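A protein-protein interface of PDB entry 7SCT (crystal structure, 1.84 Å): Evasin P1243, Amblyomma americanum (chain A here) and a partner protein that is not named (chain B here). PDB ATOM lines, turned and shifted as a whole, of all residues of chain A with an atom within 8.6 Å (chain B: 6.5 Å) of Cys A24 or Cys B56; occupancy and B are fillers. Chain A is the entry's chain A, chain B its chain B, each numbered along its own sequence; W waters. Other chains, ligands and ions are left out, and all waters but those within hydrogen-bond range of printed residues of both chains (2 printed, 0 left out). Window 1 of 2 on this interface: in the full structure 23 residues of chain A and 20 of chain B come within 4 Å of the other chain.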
ATOM      1  N   TYR A  15     -36.901 -26.709  30.129  1.00  0.00           N
ATOM      2  CA  TYR A  15     -35.662 -26.075  29.688  1.00  0.00           C
ATOM      3  C   TYR A  15     -34.659 -27.092  29.156  1.00  0.00           C
ATOM      4  O   TYR A  15     -34.450 -28.153  29.746  1.00  0.00           O
ATOM      5  CB  TYR A  15     -35.037 -25.271  30.826  1.00  0.00           C
ATOM      6  CG  TYR A  15     -33.977 -24.305  30.351  1.00  0.00           C
ATOM      7  CD1 TYR A  15     -34.325 -23.061  29.848  1.00  0.00           C
ATOM      8  CD2 TYR A  15     -32.627 -24.632  30.409  1.00  0.00           C
ATOM      9  CE1 TYR A  15     -33.363 -22.168  29.411  1.00  0.00           C
ATOM     10  CE2 TYR A  15     -31.654 -23.742  29.974  1.00  0.00           C
ATOM     11  CZ  TYR A  15     -32.034 -22.508  29.478  1.00  0.00           C
ATOM     12  OH  TYR A  15     -31.092 -21.600  29.045  1.00  0.00           O
ATOM     13  N   GLU A  19     -29.923 -27.132  23.753  1.00  0.00           N
ATOM     14  CA  GLU A  19     -30.418 -26.124  22.813  1.00  0.00           C
ATOM     15  C   GLU A  19     -29.928 -24.726  23.163  1.00  0.00           C
ATOM     16  O   GLU A  19     -29.560 -23.951  22.274  1.00  0.00           O
ATOM     17  CB  GLU A  19     -31.949 -26.121  22.764  1.00  0.00           C
ATOM     18  CG  GLU A  19     -32.567 -27.146  21.862  1.00  0.00           C
ATOM     19  CD  GLU A  19     -32.328 -26.811  20.404  1.00  0.00           C
ATOM     20  OE1 GLU A  19     -31.637 -27.594  19.728  1.00  0.00           O
ATOM     21  OE2 GLU A  19     -32.803 -25.749  19.941  1.00  0.00           O
ATOM     22  N   ALA A  20     -29.944 -24.372  24.449  1.00  0.00           N
ATOM     23  CA  ALA A  20     -29.595 -23.015  24.850  1.00  0.00           C
ATOM     24  C   ALA A  20     -28.099 -22.745  24.790  1.00  0.00           C
ATOM     25  O   ALA A  20     -27.698 -21.579  24.688  1.00  0.00           O
ATOM     26  CB  ALA A  20     -30.103 -22.745  26.270  1.00  0.00           C
ATOM     27  N   ARG A  21     -27.279 -23.802  24.816  1.00  0.00           N
ATOM     28  CA  ARG A  21     -25.866 -23.667  25.159  1.00  0.00           C
ATOM     29  C   ARG A  21     -25.175 -22.613  24.298  1.00  0.00           C
ATOM     30  O   ARG A  21     -24.474 -21.737  24.813  1.00  0.00           O
ATOM     31  CB  ARG A  21     -25.172 -25.024  25.014  1.00  0.00           C
ATOM     32  CG  ARG A  21     -23.726 -25.031  25.458  1.00  0.00           C
ATOM     33  CD  ARG A  21     -23.675 -24.873  26.980  1.00  0.00           C
ATOM     34  NE  ARG A  21     -24.214 -26.044  27.678  1.00  0.00           N
ATOM     35  CZ  ARG A  21     -24.556 -26.065  28.966  1.00  0.00           C
ATOM     36  NH1 ARG A  21     -24.429 -24.970  29.710  1.00  0.00           N
ATOM     37  NH2 ARG A  21     -25.038 -27.177  29.507  1.00  0.00           N
ATOM     38  N   CYS A  22     -25.373 -22.671  22.982  1.00  0.00           N
ATOM     39  CA  CYS A  22     -24.730 -21.735  22.076  1.00  0.00           C
ATOM     40  C   CYS A  22     -25.707 -20.713  21.522  1.00  0.00           C
ATOM     41  O   CYS A  22     -25.410 -20.052  20.522  1.00  0.00           O
ATOM     42  CB  CYS A  22     -24.040 -22.492  20.941  1.00  0.00           C
ATOM     43  SG  CYS A  22     -22.533 -23.305  21.549  1.00  0.00           S
ATOM     44  N   ALA A  23     -26.864 -20.558  22.165  1.00  0.00           N
ATOM     45  CA  ALA A  23     -27.886 -19.619  21.713  1.00  0.00           C
ATOM     46  C   ALA A  23     -27.850 -18.322  22.514  1.00  0.00           C
ATOM     47  O   ALA A  23     -28.890 -17.734  22.806  1.00  0.00           O
ATOM     48  CB  ALA A  23     -29.265 -20.271  21.780  1.00  0.00           C
ATOM     49  N   CYS A  24     -26.668 -17.851  22.894  1.00  0.00           N
ATOM     50  CA  CYS A  24     -26.588 -16.565  23.584  1.00  0.00           C
ATOM     51  C   CYS A  24     -26.017 -15.530  22.615  1.00  0.00           C
ATOM     52  O   CYS A  24     -25.373 -15.901  21.634  1.00  0.00           O
ATOM     53  CB  CYS A  24     -25.724 -16.640  24.855  1.00  0.00           C
ATOM     54  SG  CYS A  24     -23.912 -16.479  24.653  1.00  0.00           S
ATOM     55  N   PRO A  25     -26.282 -14.241  22.800  1.00  0.00           N
ATOM     56  CA  PRO A  25     -25.682 -13.246  21.904  1.00  0.00           C
ATOM     57  C   PRO A  25     -24.195 -13.073  22.167  1.00  0.00           C
ATOM     58  O   PRO A  25     -23.688 -13.333  23.264  1.00  0.00           O
ATOM     59  CB  PRO A  25     -26.450 -11.958  22.221  1.00  0.00           C
ATOM     60  CG  PRO A  25     -26.999 -12.168  23.580  1.00  0.00           C
ATOM     61  CD  PRO A  25     -27.298 -13.644  23.675  1.00  0.00           C
ATOM     62  N   ALA A  26     -23.498 -12.592  21.138  1.00  0.00           N
ATOM     63  CA  ALA A  26     -22.057 -12.385  21.212  1.00  0.00           C
ATOM     64  C   ALA A  26     -21.711 -10.998  20.687  1.00  0.00           C
ATOM     65  O   ALA A  26     -22.388 -10.473  19.796  1.00  0.00           O
ATOM     66  CB  ALA A  26     -21.313 -13.464  20.408  1.00  0.00           C
ATOM     67  N   ARG A  27     -20.650 -10.407  21.239  1.00  0.00           N
ATOM     68  CA  ARG A  27     -20.208  -9.096  20.784  1.00  0.00           C
ATOM     69  C   ARG A  27     -19.641  -9.207  19.369  1.00  0.00           C
ATOM     70  O   ARG A  27     -18.916 -10.158  19.048  1.00  0.00           O
ATOM     71  CB  ARG A  27     -19.168  -8.502  21.745  1.00  0.00           C
ATOM     72  CG  ARG A  27     -18.918  -7.002  21.510  1.00  0.00           C
ATOM     73  CD  ARG A  27     -18.286  -6.252  22.713  1.00  0.00           C
ATOM     74  NE  ARG A  27     -19.105  -6.249  23.932  1.00  0.00           N
ATOM     75  CZ  ARG A  27     -20.157  -5.452  24.137  1.00  0.00           C
ATOM     76  NH1 ARG A  27     -20.545  -4.597  23.196  1.00  0.00           N
ATOM     77  NH2 ARG A  27     -20.837  -5.514  25.280  1.00  0.00           N
ATOM     78  N   HIS A  28     -20.027  -8.266  18.504  1.00  0.00           N
ATOM     79  CA  HIS A  28     -19.557  -8.188  17.123  1.00  0.00           C
ATOM     80  C   HIS A  28     -18.690  -6.944  16.945  1.00  0.00           C
ATOM     81  O   HIS A  28     -18.691  -6.035  17.775  1.00  0.00           O
ATOM     82  CB  HIS A  28     -20.738  -8.128  16.133  1.00  0.00           C
ATOM     83  CG  HIS A  28     -21.455  -9.431  15.952  1.00  0.00           C
ATOM     84  ND1 HIS A  28     -21.899 -10.191  17.013  1.00  0.00           N
ATOM     85  CD2 HIS A  28     -21.773 -10.126  14.831  1.00  0.00           C
ATOM     86  CE1 HIS A  28     -22.470 -11.293  16.554  1.00  0.00           C
ATOM     87  NE2 HIS A  28     -22.403 -11.281  15.233  1.00  0.00           N
ATOM     88  N   LEU A  39     -18.682 -11.026  13.134  1.00  0.00           N
ATOM     89  CA  LEU A  39     -17.954 -11.611  14.246  1.00  0.00           C
ATOM     90  C   LEU A  39     -16.455 -11.531  13.995  1.00  0.00           C
ATOM     91  O   LEU A  39     -15.996 -11.728  12.872  1.00  0.00           O
ATOM     92  CB  LEU A  39     -18.356 -13.074  14.440  1.00  0.00           C
ATOM     93  CG  LEU A  39     -17.998 -13.711  15.780  1.00  0.00           C
ATOM     94  CD1 LEU A  39     -18.855 -13.101  16.867  1.00  0.00           C
ATOM     95  CD2 LEU A  39     -18.212 -15.218  15.710  1.00  0.00           C
ATOM     96  N   TYR A  44     -17.324 -17.999  19.505  1.00  0.00           N
ATOM     97  CA  TYR A  44     -17.827 -17.115  20.555  1.00  0.00           C
ATOM     98  C   TYR A  44     -18.110 -17.913  21.818  1.00  0.00           C
ATOM     99  O   TYR A  44     -18.285 -19.133  21.784  1.00  0.00           O
ATOM    100  CB  TYR A  44     -19.075 -16.363  20.083  1.00  0.00           C
ATOM    101  CG  TYR A  44     -20.236 -17.269  19.736  1.00  0.00           C
ATOM    102  CD1 TYR A  44     -20.259 -17.959  18.531  1.00  0.00           C
ATOM    103  CD2 TYR A  44     -21.319 -17.423  20.605  1.00  0.00           C
ATOM    104  CE1 TYR A  44     -21.326 -18.786  18.194  1.00  0.00           C
ATOM    105  CE2 TYR A  44     -22.392 -18.251  20.276  1.00  0.00           C
ATOM    106  CZ  TYR A  44     -22.392 -18.924  19.063  1.00  0.00           C
ATOM    107  OH  TYR A  44     -23.436 -19.750  18.716  1.00  0.00           O
ATOM    108  N   PHE A  45     -18.161 -17.192  22.944  1.00  0.00           N
ATOM    109  CA  PHE A  45     -18.304 -17.751  24.277  1.00  0.00           C
ATOM    110  C   PHE A  45     -19.739 -17.606  24.773  1.00  0.00           C
ATOM    111  O   PHE A  45     -20.329 -16.529  24.665  1.00  0.00           O
ATOM    112  CB  PHE A  45     -17.385 -16.980  25.203  1.00  0.00           C
ATOM    113  CG  PHE A  45     -15.981 -17.409  25.120  1.00  0.00           C
ATOM    114  CD1 PHE A  45     -15.628 -18.723  25.358  1.00  0.00           C
ATOM    115  CD2 PHE A  45     -15.014 -16.520  24.672  1.00  0.00           C
ATOM    116  CE1 PHE A  45     -14.313 -19.122  25.259  1.00  0.00           C
ATOM    117  CE2 PHE A  45     -13.689 -16.916  24.557  1.00  0.00           C
ATOM    118  CZ  PHE A  45     -13.338 -18.219  24.852  1.00  0.00           C
ATOM    119  N   CYS A  46     -20.282 -18.680  25.346  1.00  0.00           N
ATOM    120  CA  CYS A  46     -21.633 -18.677  25.909  1.00  0.00           C
ATOM    121  C   CYS A  46     -21.611 -19.545  27.152  1.00  0.00           C
ATOM    122  O   CYS A  46     -21.592 -20.776  27.045  1.00  0.00           O
ATOM    123  CB  CYS A  46     -22.678 -19.213  24.933  1.00  0.00           C
ATOM    124  SG  CYS A  46     -23.205 -18.112  23.635  1.00  0.00           S
ATOM    125  N   ASN A  47     -21.627 -18.910  28.317  1.00  0.00           N
ATOM    126  CA  ASN A  47     -21.808 -19.619  29.579  1.00  0.00           C
ATOM    127  C   ASN A  47     -20.692 -20.643  29.792  1.00  0.00           C
ATOM    128  O   ASN A  47     -20.938 -21.789  30.170  1.00  0.00           O
ATOM    129  CB  ASN A  47     -23.185 -20.292  29.607  1.00  0.00           C
ATOM    130  CG  ASN A  47     -24.331 -19.282  29.526  1.00  0.00           C
ATOM    131  OD1 ASN A  47     -25.191 -19.360  28.638  1.00  0.00           O
ATOM    132  ND2 ASN A  47     -24.330 -18.319  30.440  1.00  0.00           N
ATOM    133  N   GLY A  48     -19.454 -20.246  29.506  1.00  0.00           N
ATOM    134  CA  GLY A  48     -18.343 -21.170  29.648  1.00  0.00           C
ATOM    135  C   GLY A  48     -18.211 -22.223  28.565  1.00  0.00           C
ATOM    136  O   GLY A  48     -17.382 -23.128  28.701  1.00  0.00           O
ATOM    137  N   THR A  49     -19.012 -22.159  27.510  1.00  0.00           N
ATOM    138  CA  THR A  49     -18.850 -23.022  26.344  1.00  0.00           C
ATOM    139  C   THR A  49     -18.232 -22.225  25.208  1.00  0.00           C
ATOM    140  O   THR A  49     -18.570 -21.059  24.997  1.00  0.00           O
ATOM    141  CB  THR A  49     -20.192 -23.623  25.898  1.00  0.00           C
ATOM    142  OG1 THR A  49     -20.652 -24.541  26.897  1.00  0.00           O
ATOM    143  CG2 THR A  49     -20.079 -24.363  24.554  1.00  0.00           C
ATOM    144  N   CYS A  51     -18.272 -21.780  21.421  1.00  0.00           N
ATOM    145  CA  CYS A  51     -19.230 -22.066  20.361  1.00  0.00           C
ATOM    146  C   CYS A  51     -18.654 -21.711  18.992  1.00  0.00           C
ATOM    147  O   CYS A  51     -17.777 -20.854  18.858  1.00  0.00           O
ATOM    148  CB  CYS A  51     -20.527 -21.283  20.590  1.00  0.00           C
ATOM    149  SG  CYS A  51     -21.383 -21.727  22.133  1.00  0.00           S
ATOM    150  N   CYS B  17     -25.242  -9.625  18.964  1.00  0.00           N
ATOM    151  CA  CYS B  17     -26.135 -10.257  18.011  1.00  0.00           C
ATOM    152  C   CYS B  17     -26.097 -11.758  18.228  1.00  0.00           C
ATOM    153  O   CYS B  17     -25.090 -12.300  18.677  1.00  0.00           O
ATOM    154  CB  CYS B  17     -25.708  -9.958  16.559  1.00  0.00           C
ATOM    155  SG  CYS B  17     -26.061  -8.286  15.997  1.00  0.00           S
ATOM    156  N   CYS B  18     -27.184 -12.425  17.844  1.00  0.00           N
ATOM    157  CA  CYS B  18     -27.347 -13.865  18.001  1.00  0.00           C
ATOM    158  C   CYS B  18     -26.800 -14.623  16.796  1.00  0.00           C
ATOM    159  O   CYS B  18     -26.899 -14.147  15.666  1.00  0.00           O
ATOM    160  CB  CYS B  18     -28.830 -14.190  18.147  1.00  0.00           C
ATOM    161  SG  CYS B  18     -29.472 -13.516  19.677  1.00  0.00           S
ATOM    162  N   LEU B  19     -26.240 -15.819  17.048  1.00  0.00           N
ATOM    163  CA  LEU B  19     -25.744 -16.684  15.976  1.00  0.00           C
ATOM    164  C   LEU B  19     -26.522 -17.989  15.794  1.00  0.00           C
ATOM    165  O   LEU B  19     -26.315 -18.684  14.783  1.00  0.00           O
ATOM    166  CB  LEU B  19     -24.265 -17.013  16.223  1.00  0.00           C
ATOM    167  CG  LEU B  19     -23.346 -15.793  16.177  1.00  0.00           C
ATOM    168  CD1 LEU B  19     -23.021 -15.318  17.586  1.00  0.00           C
ATOM    169  CD2 LEU B  19     -22.057 -16.134  15.426  1.00  0.00           C
ATOM    170  N   LYS B  20     -27.359 -18.366  16.753  1.00  0.00           N
ATOM    171  CA  LYS B  20     -28.129 -19.607  16.723  1.00  0.00           C
ATOM    172  C   LYS B  20     -29.401 -19.352  17.520  1.00  0.00           C
ATOM    173  O   LYS B  20     -29.361 -18.641  18.521  1.00  0.00           O
ATOM    174  CB  LYS B  20     -27.379 -20.797  17.368  1.00  0.00           C
ATOM    175  CG  LYS B  20     -28.221 -22.087  17.423  1.00  0.00           C
ATOM    176  CD  LYS B  20     -27.521 -23.254  18.130  1.00  0.00           C
ATOM    177  CE  LYS B  20     -28.220 -23.504  19.480  1.00  0.00           C
ATOM    178  NZ  LYS B  20     -27.370 -24.209  20.519  1.00  0.00           N
ATOM    179  N   TYR B  21     -30.522 -19.935  17.080  1.00  0.00           N
ATOM    180  CA  TYR B  21     -31.794 -19.829  17.793  1.00  0.00           C
ATOM    181  C   TYR B  21     -31.991 -21.016  18.725  1.00  0.00           C
ATOM    182  O   TYR B  21     -31.686 -22.159  18.369  1.00  0.00           O
ATOM    183  CB  TYR B  21     -32.989 -19.810  16.840  1.00  0.00           C
ATOM    184  CG  TYR B  21     -33.131 -18.614  15.936  1.00  0.00           C
ATOM    185  CD1 TYR B  21     -32.948 -17.321  16.409  1.00  0.00           C
ATOM    186  CD2 TYR B  21     -33.493 -18.785  14.599  1.00  0.00           C
ATOM    187  CE1 TYR B  21     -33.092 -16.233  15.561  1.00  0.00           C
ATOM    188  CE2 TYR B  21     -33.642 -17.714  13.759  1.00  0.00           C
ATOM    189  CZ  TYR B  21     -33.455 -16.440  14.244  1.00  0.00           C
ATOM    190  OH  TYR B  21     -33.612 -15.369  13.386  1.00  0.00           O
ATOM    191  N   TYR B  22     -32.553 -20.741  19.899  1.00  0.00           N
ATOM    192  CA  TYR B  22     -33.121 -21.776  20.753  1.00  0.00           C
ATOM    193  C   TYR B  22     -34.444 -22.223  20.139  1.00  0.00           C
ATOM    194  O   TYR B  22     -35.418 -21.462  20.143  1.00  0.00           O
ATOM    195  CB  TYR B  22     -33.307 -21.207  22.156  1.00  0.00           C
ATOM    196  CG  TYR B  22     -33.874 -22.162  23.174  1.00  0.00           C
ATOM    197  CD1 TYR B  22     -33.039 -22.961  23.943  1.00  0.00           C
ATOM    198  CD2 TYR B  22     -35.241 -22.269  23.367  1.00  0.00           C
ATOM    199  CE1 TYR B  22     -33.555 -23.839  24.877  1.00  0.00           C
ATOM    200  CE2 TYR B  22     -35.765 -23.145  24.283  1.00  0.00           C
ATOM    201  CZ  TYR B  22     -34.921 -23.927  25.040  1.00  0.00           C
ATOM    202  OH  TYR B  22     -35.442 -24.798  25.968  1.00  0.00           O
ATOM    203  N   GLU B  23     -34.492 -23.452  19.613  1.00  0.00           N
ATOM    204  CA  GLU B  23     -35.583 -23.842  18.724  1.00  0.00           C
ATOM    205  C   GLU B  23     -36.831 -24.344  19.457  1.00  0.00           C
ATOM    206  O   GLU B  23     -37.827 -24.660  18.798  1.00  0.00           O
ATOM    207  CB  GLU B  23     -35.130 -24.935  17.746  1.00  0.00           C
ATOM    208  CG  GLU B  23     -34.039 -24.601  16.715  1.00  0.00           C
ATOM    209  CD  GLU B  23     -34.446 -23.565  15.680  1.00  0.00           C
ATOM    210  OE1 GLU B  23     -35.650 -23.455  15.377  1.00  0.00           O
ATOM    211  OE2 GLU B  23     -33.537 -22.949  15.077  1.00  0.00           O
ATOM    212  N   LEU B  42     -28.531 -12.488  12.031  1.00  0.00           N
ATOM    213  CA  LEU B  42     -29.621 -13.386  12.428  1.00  0.00           C
ATOM    214  C   LEU B  42     -30.521 -12.612  13.377  1.00  0.00           C
ATOM    215  O   LEU B  42     -30.238 -12.543  14.584  1.00  0.00           O
ATOM    216  CB  LEU B  42     -29.090 -14.644  13.110  1.00  0.00           C
ATOM    217  CG  LEU B  42     -30.151 -15.708  13.372  1.00  0.00           C
ATOM    218  CD1 LEU B  42     -30.570 -16.379  12.051  1.00  0.00           C
ATOM    219  CD2 LEU B  42     -29.635 -16.728  14.389  1.00  0.00           C
ATOM    220  N   ALA B  44     -33.105 -11.552  16.046  1.00  0.00           N
ATOM    221  CA  ALA B  44     -33.541 -12.378  17.161  1.00  0.00           C
ATOM    222  C   ALA B  44     -34.270 -11.541  18.200  1.00  0.00           C
ATOM    223  O   ALA B  44     -34.027 -10.339  18.357  1.00  0.00           O
ATOM    224  CB  ALA B  44     -32.370 -13.071  17.872  1.00  0.00           C
ATOM    225  N   ILE B  45     -35.125 -12.227  18.946  1.00  0.00           N
ATOM    226  CA  ILE B  45     -35.621 -11.762  20.240  1.00  0.00           C
ATOM    227  C   ILE B  45     -34.817 -12.481  21.306  1.00  0.00           C
ATOM    228  O   ILE B  45     -34.705 -13.712  21.286  1.00  0.00           O
ATOM    229  CB  ILE B  45     -37.122 -12.050  20.404  1.00  0.00           C
ATOM    230  CG1 ILE B  45     -37.945 -11.358  19.303  1.00  0.00           C
ATOM    231  CG2 ILE B  45     -37.609 -11.641  21.808  1.00  0.00           C
ATOM    232  CD1 ILE B  45     -37.860  -9.847  19.312  1.00  0.00           C
ATOM    233  N   ILE B  46     -34.239 -11.722  22.222  1.00  0.00           N
ATOM    234  CA  ILE B  46     -33.441 -12.276  23.298  1.00  0.00           C
ATOM    235  C   ILE B  46     -34.276 -12.266  24.569  1.00  0.00           C
ATOM    236  O   ILE B  46     -34.628 -11.193  25.075  1.00  0.00           O
ATOM    237  CB  ILE B  46     -32.135 -11.493  23.487  1.00  0.00           C
ATOM    238  CG1 ILE B  46     -31.271 -11.583  22.215  1.00  0.00           C
ATOM    239  CG2 ILE B  46     -31.365 -12.016  24.680  1.00  0.00           C
ATOM    240  CD1 ILE B  46     -30.176 -10.530  22.180  1.00  0.00           C
ATOM    241  N   PHE B  47     -34.569 -13.450  25.105  1.00  0.00           N
ATOM    242  CA  PHE B  47     -35.204 -13.548  26.421  1.00  0.00           C
ATOM    243  C   PHE B  47     -34.141 -13.712  27.490  1.00  0.00           C
ATOM    244  O   PHE B  47     -33.156 -14.419  27.287  1.00  0.00           O
ATOM    245  CB  PHE B  47     -36.165 -14.729  26.485  1.00  0.00           C
ATOM    246  CG  PHE B  47     -37.362 -14.556  25.616  1.00  0.00           C
ATOM    247  CD1 PHE B  47     -38.344 -13.636  25.959  1.00  0.00           C
ATOM    248  CD2 PHE B  47     -37.498 -15.281  24.443  1.00  0.00           C
ATOM    249  CE1 PHE B  47     -39.461 -13.459  25.142  1.00  0.00           C
ATOM    250  CE2 PHE B  47     -38.617 -15.099  23.614  1.00  0.00           C
ATOM    251  CZ  PHE B  47     -39.597 -14.192  23.970  1.00  0.00           C
ATOM    252  N   ARG B  53     -29.587 -15.930  32.140  1.00  0.00           N
ATOM    253  CA  ARG B  53     -29.110 -16.429  30.857  1.00  0.00           C
ATOM    254  C   ARG B  53     -29.839 -15.687  29.749  1.00  0.00           C
ATOM    255  O   ARG B  53     -31.026 -15.380  29.874  1.00  0.00           O
ATOM    256  CB  ARG B  53     -29.347 -17.935  30.712  1.00  0.00           C
ATOM    257  CG  ARG B  53     -28.615 -18.779  31.748  1.00  0.00           C
ATOM    258  CD  ARG B  53     -27.170 -18.326  31.887  1.00  0.00           C
ATOM    259  NE  ARG B  53     -26.323 -19.220  32.689  1.00  0.00           N
ATOM    260  CZ  ARG B  53     -26.045 -20.493  32.403  1.00  0.00           C
ATOM    261  NH1 ARG B  53     -26.516 -21.069  31.302  1.00  0.00           N
ATOM    262  NH2 ARG B  53     -25.262 -21.192  33.218  1.00  0.00           N
ATOM    263  N   GLU B  54     -29.121 -15.401  28.669  1.00  0.00           N
ATOM    264  CA  GLU B  54     -29.679 -14.734  27.497  1.00  0.00           C
ATOM    265  C   GLU B  54     -29.935 -15.779  26.424  1.00  0.00           C
ATOM    266  O   GLU B  54     -29.002 -16.463  26.004  1.00  0.00           O
ATOM    267  CB  GLU B  54     -28.704 -13.684  26.980  1.00  0.00           C
ATOM    268  CG  GLU B  54     -28.601 -12.428  27.794  1.00  0.00           C
ATOM    269  CD  GLU B  54     -27.798 -11.375  27.055  1.00  0.00           C
ATOM    270  OE1 GLU B  54     -28.394 -10.353  26.649  1.00  0.00           O
ATOM    271  OE2 GLU B  54     -26.559 -11.542  26.935  1.00  0.00           O
ATOM    272  N   VAL B  55     -31.184 -15.902  25.987  1.00  0.00           N
ATOM    273  CA  VAL B  55     -31.583 -16.948  25.045  1.00  0.00           C
ATOM    274  C   VAL B  55     -32.072 -16.297  23.751  1.00  0.00           C
ATOM    275  O   VAL B  55     -33.083 -15.586  23.755  1.00  0.00           O
ATOM    276  CB  VAL B  55     -32.670 -17.858  25.634  1.00  0.00           C
ATOM    277  CG1 VAL B  55     -33.044 -18.936  24.613  1.00  0.00           C
ATOM    278  CG2 VAL B  55     -32.204 -18.478  26.960  1.00  0.00           C
ATOM    279  N   CYS B  56     -31.368 -16.563  22.653  1.00  0.00           N
ATOM    280  CA  CYS B  56     -31.770 -16.085  21.331  1.00  0.00           C
ATOM    281  C   CYS B  56     -32.942 -16.888  20.770  1.00  0.00           C
ATOM    282  O   CYS B  56     -32.929 -18.123  20.786  1.00  0.00           O
ATOM    283  CB  CYS B  56     -30.582 -16.208  20.367  1.00  0.00           C
ATOM    284  SG  CYS B  56     -29.178 -15.167  20.866  1.00  0.00           S
ATOM    285  N   THR B  57     -33.935 -16.187  20.202  1.00  0.00           N
ATOM    286  CA  THR B  57     -35.108 -16.869  19.655  1.00  0.00           C
ATOM    287  C   THR B  57     -35.496 -16.249  18.321  1.00  0.00           C
ATOM    288  O   THR B  57     -35.083 -15.134  17.976  1.00  0.00           O
ATOM    289  CB  THR B  57     -36.297 -16.825  20.628  1.00  0.00           C
ATOM    290  OG1 THR B  57     -36.707 -15.458  20.785  1.00  0.00           O
ATOM    291  CG2 THR B  57     -35.898 -17.403  22.007  1.00  0.00           C
ATOM    292  N   ASN B  58     -36.282 -17.005  17.559  1.00  0.00           N
ATOM    293  CA  ASN B  58     -36.706 -16.568  16.232  1.00  0.00           C
ATOM    294  C   ASN B  58     -37.913 -15.629  16.315  1.00  0.00           C
ATOM    295  O   ASN B  58     -38.978 -16.049  16.779  1.00  0.00           O
ATOM    296  CB  ASN B  58     -37.034 -17.790  15.380  1.00  0.00           C
ATOM    297  CG  ASN B  58     -37.234 -17.446  13.936  1.00  0.00           C
ATOM    298  OD1 ASN B  58     -37.666 -16.342  13.614  1.00  0.00           O
ATOM    299  ND2 ASN B  58     -36.935 -18.399  13.040  1.00  0.00           N
HETATM  300  O   HOH W   1     -26.088 -17.187  19.406  1.00  0.00           O
HETATM  301  O   HOH W   2     -28.105 -19.000  26.397  1.00  0.00           O
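N of Ala A26 sits at hydrogen-bond distance from O of Cys B17, 2.9 Å away. O of Glu B54 sits close to O of Ala A23 (3.4 Å). The backbone carbonyl oxygen of Ala A23 sits at hydrogen-bond distance from the backbone NH of Cys B56, at 2.7 Å. The side-chain carboxylate (OE2) of Glu A19 is in hydrogen-bond range of the backbone NH (N) of Glu B23, at 2.9 Å. N of Pro A25 sits close to SG of Cys B56, at 3.6 Å. The side-chain amino group (NZ) of Lys B20 sits at hydrogen-bond distance from the backbone carbonyl oxygen (O) of Glu A19 (2.8 Å). The side-chain amide nitrogen (ND2) of Asn A47 sits close to the guanidinium group (NE) of Arg B53, 3.1 Å away.
SG of Cys B56 forms a disulfide with SG of Cys B18 (2.1 Å). SG of Cys A51 forms a disulfide with SG of Cys A22 (2.0 Å). O of Ala A26 lies within hydrogen-bond range of ND1 of His A28, at 2.8 Å. O of Tyr A44 sits at hydrogen-bond distance from N of Cys A51. The backbone NH (N) of Tyr B22 is in hydrogen-bond range of the backbone carbonyl oxygen (O) of Cys B56, at 2.8 Å. The backbone carbonyl oxygen of Phe B47 lies within hydrogen-bond range of the backbone NH of Val B55, at 2.8 Å.
Among the printed residues, pairs that only touch across the chains: Tyr A15 with Tyr B22, Tyr A15 with Val B55, Glu A19 with Tyr B22, Ala A20 with Tyr B22, Cys A22 with Lys B20, Ala A23 with Lys B20, Ala A23 with Tyr B22, Ala A23 with Val B55, Cys A24 with Glu B54, Cys A24 with Cys B56, Pro A25 with Cys B17, Pro A25 with Ile B46, Pro A25 with Glu B54, Ala A26 with Leu B19, His A28 with Cys B17, Leu A39 with Leu B19 and Tyr A44 with Leu B19.
Of the printed residues of chain B, Cys A24 touches Glu B54 and Cys B56. Of chain A, only Ala A23 (2.7 Å), Cys A24 (3.6 Å) and Pro A25 (3.6 Å) come within 4 Å of Cys B56. No residue of chain A comes within 4 Å of Thr B57. Printed residues of chain B within 4 Å of Asn A47: Arg B53 (3.1 Å). Printed residues of chain A within 4 Å of Val B55: Tyr A15 and Ala A23. Leu B42 touches none of the printed residues of chain A. The nearest residue of chain A that does not touch Cys B56 is Cys A22 (6.2 Å). The nearest printed residue of chain B that does not touch Glu A19 is Tyr B21 (4.1 Å).
Of the 19 printed residues of chain A, 12 touch a printed residue of chain B. Printed residues of chain A that touch a printed residue of chain B: Tyr A15, Glu A19, Ala A20, Cys A22, Ala A23, Cys A24, Pro A25, Ala A26, His A28, Leu A39, Tyr A44 and Asn A47. Hydrophobic or aromatic side chains of chain A within 4 Å of the printed part of chain B: Tyr A15, Ala A20, Ala A23, Pro A25, Ala A26, His A28, Leu A39 and Tyr A44. Along chain A the printed residues that touch a printed residue of chain B span positions 15 to 47. Among the printed residues, 24 pairs touch across the chains.
Water W1 lies within hydrogen-bond range of the backbone carbonyl oxygen of Cys A24 (2.7 Å), the backbone NH of Leu B19 (2.7 Å), the backbone carbonyl oxygen of Cys A22 (3.1 Å) and the backbone NH of Lys B20 (3.2 Å). Water W2 lies within hydrogen-bond range of the backbone carbonyl oxygen of Glu B54 (2.7 Å) and the backbone carbonyl oxygen of Ala A20 (3.1 Å).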
